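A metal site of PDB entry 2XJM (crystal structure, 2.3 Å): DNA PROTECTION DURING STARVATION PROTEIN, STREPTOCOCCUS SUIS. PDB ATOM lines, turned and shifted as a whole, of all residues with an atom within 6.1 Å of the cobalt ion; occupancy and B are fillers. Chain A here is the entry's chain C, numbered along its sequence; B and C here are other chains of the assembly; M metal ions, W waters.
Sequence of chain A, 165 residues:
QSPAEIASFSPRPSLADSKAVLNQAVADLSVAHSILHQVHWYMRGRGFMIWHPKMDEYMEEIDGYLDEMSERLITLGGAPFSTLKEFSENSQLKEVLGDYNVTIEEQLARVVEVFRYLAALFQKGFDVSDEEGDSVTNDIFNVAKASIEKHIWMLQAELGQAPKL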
ATOM      1  N   ASP A  67      -3.599  17.779 -23.943  1.00  0.00           N
ATOM      2  CA  ASP A  67      -2.550  18.730 -23.627  1.00  0.00           C
ATOM      3  C   ASP A  67      -2.308  18.878 -22.122  1.00  0.00           C
ATOM      4  O   ASP A  67      -1.177  18.960 -21.661  1.00  0.00           O
ATOM      5  CB  ASP A  67      -2.774  20.058 -24.342  1.00  0.00           C
ATOM      6  CG  ASP A  67      -1.512  20.917 -24.350  1.00  0.00           C
ATOM      7  OD1 ASP A  67      -1.525  21.995 -23.664  1.00  0.00           O
ATOM      8  OD2 ASP A  67      -0.499  20.498 -24.991  1.00  0.00           O
ATOM      9  N   GLU A  71       1.272  17.349 -20.316  1.00  0.00           N
ATOM     10  CA  GLU A  71       1.984  18.357 -19.574  1.00  0.00           C
ATOM     11  C   GLU A  71       2.096  18.072 -18.091  1.00  0.00           C
ATOM     12  O   GLU A  71       3.074  18.446 -17.480  1.00  0.00           O
ATOM     13  CB  GLU A  71       1.422  19.743 -19.863  1.00  0.00           C
ATOM     14  CG  GLU A  71       1.933  20.173 -21.192  1.00  0.00           C
ATOM     15  CD  GLU A  71       1.214  21.333 -21.790  1.00  0.00           C
ATOM     16  OE1 GLU A  71       0.503  22.093 -21.065  1.00  0.00           O
ATOM     17  OE2 GLU A  71       1.401  21.462 -23.026  1.00  0.00           O
ATOM     18  N   HIS B  37       3.660  19.215 -31.961  1.00  0.00           N
ATOM     19  CA  HIS B  37       3.270  18.886 -30.601  1.00  0.00           C
ATOM     20  C   HIS B  37       4.493  18.390 -29.809  1.00  0.00           C
ATOM     21  O   HIS B  37       4.725  18.829 -28.675  1.00  0.00           O
ATOM     22  CB  HIS B  37       2.148  17.839 -30.643  1.00  0.00           C
ATOM     23  CG  HIS B  37       1.004  18.165 -29.745  1.00  0.00           C
ATOM     24  ND1 HIS B  37       1.116  19.041 -28.689  1.00  0.00           N
ATOM     25  CD2 HIS B  37      -0.276  17.718 -29.732  1.00  0.00           C
ATOM     26  CE1 HIS B  37      -0.044  19.119 -28.055  1.00  0.00           C
ATOM     27  NE2 HIS B  37      -0.903  18.329 -28.662  1.00  0.00           N
ATOM     28  N   HIS B  40       6.722  21.248 -29.093  1.00  0.00           N
ATOM     29  CA  HIS B  40       6.012  21.965 -28.021  1.00  0.00           C
ATOM     30  C   HIS B  40       6.328  21.345 -26.644  1.00  0.00           C
ATOM     31  O   HIS B  40       6.743  22.046 -25.714  1.00  0.00           O
ATOM     32  CB  HIS B  40       4.524  21.864 -28.343  1.00  0.00           C
ATOM     33  CG  HIS B  40       3.609  22.524 -27.366  1.00  0.00           C
ATOM     34  ND1 HIS B  40       3.437  23.885 -27.302  1.00  0.00           N
ATOM     35  CD2 HIS B  40       2.702  21.995 -26.511  1.00  0.00           C
ATOM     36  CE1 HIS B  40       2.519  24.176 -26.409  1.00  0.00           C
ATOM     37  NE2 HIS B  40       2.050  23.037 -25.911  1.00  0.00           N
ATOM     38  N   TRP B  41       6.143  20.032 -26.520  1.00  0.00           N
ATOM     39  CA  TRP B  41       6.372  19.332 -25.257  1.00  0.00           C
ATOM     40  C   TRP B  41       7.830  19.216 -24.793  1.00  0.00           C
ATOM     41  O   TRP B  41       8.097  19.399 -23.592  1.00  0.00           O
ATOM     42  CB  TRP B  41       5.753  17.941 -25.324  1.00  0.00           C
ATOM     43  CG  TRP B  41       4.271  17.913 -25.340  1.00  0.00           C
ATOM     44  CD1 TRP B  41       3.399  18.809 -24.734  1.00  0.00           C
ATOM     45  CD2 TRP B  41       3.442  16.894 -25.934  1.00  0.00           C
ATOM     46  NE1 TRP B  41       2.107  18.406 -24.941  1.00  0.00           N
ATOM     47  CE2 TRP B  41       2.099  17.263 -25.687  1.00  0.00           C
ATOM     48  CE3 TRP B  41       3.706  15.743 -26.676  1.00  0.00           C
ATOM     49  CZ2 TRP B  41       1.017  16.487 -26.145  1.00  0.00           C
ATOM     50  CZ3 TRP B  41       2.626  14.974 -27.128  1.00  0.00           C
ATOM     51  CH2 TRP B  41       1.314  15.343 -26.861  1.00  0.00           C
ATOM     52  N   HIS B  52       7.396  27.930 -27.120  1.00  0.00           N
ATOM     53  CA  HIS B  52       6.432  26.959 -26.642  1.00  0.00           C
ATOM     54  C   HIS B  52       4.982  27.323 -27.007  1.00  0.00           C
ATOM     55  O   HIS B  52       4.304  26.505 -27.629  1.00  0.00           O
ATOM     56  CB  HIS B  52       6.596  26.668 -25.137  1.00  0.00           C
ATOM     57  CG  HIS B  52       5.489  25.842 -24.540  1.00  0.00           C
ATOM     58  ND1 HIS B  52       5.491  24.462 -24.576  1.00  0.00           N
ATOM     59  CD2 HIS B  52       4.358  26.207 -23.891  1.00  0.00           C
ATOM     60  CE1 HIS B  52       4.408  24.006 -23.958  1.00  0.00           C
ATOM     61  NE2 HIS B  52       3.711  25.049 -23.531  1.00  0.00           N
ATOM     62  N   ASP B  56       1.831  26.211 -30.472  1.00  0.00           N
ATOM     63  CA  ASP B  56       0.383  26.145 -30.376  1.00  0.00           C
ATOM     64  C   ASP B  56      -0.299  26.851 -31.543  1.00  0.00           C
ATOM     65  O   ASP B  56      -1.199  26.293 -32.137  1.00  0.00           O
ATOM     66  CB  ASP B  56      -0.095  26.802 -29.077  1.00  0.00           C
ATOM     67  CG  ASP B  56      -0.300  25.825 -27.970  1.00  0.00           C
ATOM     68  OD1 ASP B  56      -0.876  24.756 -28.253  1.00  0.00           O
ATOM     69  OD2 ASP B  56       0.087  26.138 -26.821  1.00  0.00           O
ATOM     70  N   LYS C 150       3.065  23.542 -12.757  1.00  0.00           N
ATOM     71  CA  LYS C 150       3.084  23.847 -14.191  1.00  0.00           C
ATOM     72  C   LYS C 150       4.090  24.956 -14.461  1.00  0.00           C
ATOM     73  O   LYS C 150       4.869  24.855 -15.405  1.00  0.00           O
ATOM     74  CB  LYS C 150       1.662  24.215 -14.677  1.00  0.00           C
ATOM     75  CG  LYS C 150       1.477  24.301 -16.194  1.00  0.00           C
ATOM     76  CD  LYS C 150      -0.012  24.336 -16.671  1.00  0.00           C
ATOM     77  CE  LYS C 150      -0.588  22.946 -17.153  1.00  0.00           C
ATOM     78  NZ  LYS C 150      -0.636  22.614 -18.696  1.00  0.00           N
ATOM     79  N   TRP C 153       7.728  23.692 -14.143  1.00  0.00           N
ATOM     80  CA  TRP C 153       8.104  23.016 -15.387  1.00  0.00           C
ATOM     81  C   TRP C 153       8.600  24.016 -16.428  1.00  0.00           C
ATOM     82  O   TRP C 153       9.719  23.885 -16.961  1.00  0.00           O
ATOM     83  CB  TRP C 153       6.963  22.147 -15.954  1.00  0.00           C
ATOM     84  CG  TRP C 153       7.058  21.997 -17.464  1.00  0.00           C
ATOM     85  CD1 TRP C 153       8.167  21.598 -18.200  1.00  0.00           C
ATOM     86  CD2 TRP C 153       6.026  22.256 -18.423  1.00  0.00           C
ATOM     87  NE1 TRP C 153       7.878  21.624 -19.539  1.00  0.00           N
ATOM     88  CE2 TRP C 153       6.573  22.006 -19.704  1.00  0.00           C
ATOM     89  CE3 TRP C 153       4.695  22.678 -18.326  1.00  0.00           C
ATOM     90  CZ2 TRP C 153       5.833  22.171 -20.877  1.00  0.00           C
ATOM     91  CZ3 TRP C 153       3.963  22.837 -19.496  1.00  0.00           C
ATOM     92  CH2 TRP C 153       4.534  22.584 -20.751  1.00  0.00           C
HETATM   93 CO    CO M   1       0.476  22.802 -24.417  1.00  0.00          CO
HETATM   94  O   HOH W   1       1.294  24.722 -22.581  1.00  0.00           O
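Water W1 lies within hydrogen-bond range of a ring nitrogen (NE2) of His 52 of chain B and the side-chain carboxylate of Glu 71.
The cobalt ion is bound by the side-chain carboxylate (OE2) of Glu 71 (2.1 Å), a ring nitrogen (NE2) of His 40 of chain B (2.2 Å), the side-chain carboxylate (OD1) of Asp 67 (2.3 Å) and the side-chain carboxylate (OD2) of Asp 67 (2.6 Å).
Slightly farther from the cobalt ion lies water W1 (2.8 Å).
The backbone carbonyl oxygen (O) of His 52 of chain B is in hydrogen-bond range of a ring nitrogen (ND1) of His 40 of chain B (2.8 Å).
The side-chain amino group of Lys 150 of chain C is in salt-bridge range of the side-chain carboxylate of Glu 71, 2.7 Å away.
The indole nitrogen of Trp 41 of chain B lies close to the side-chain carboxylate of Asp 67 (3.3 Å).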
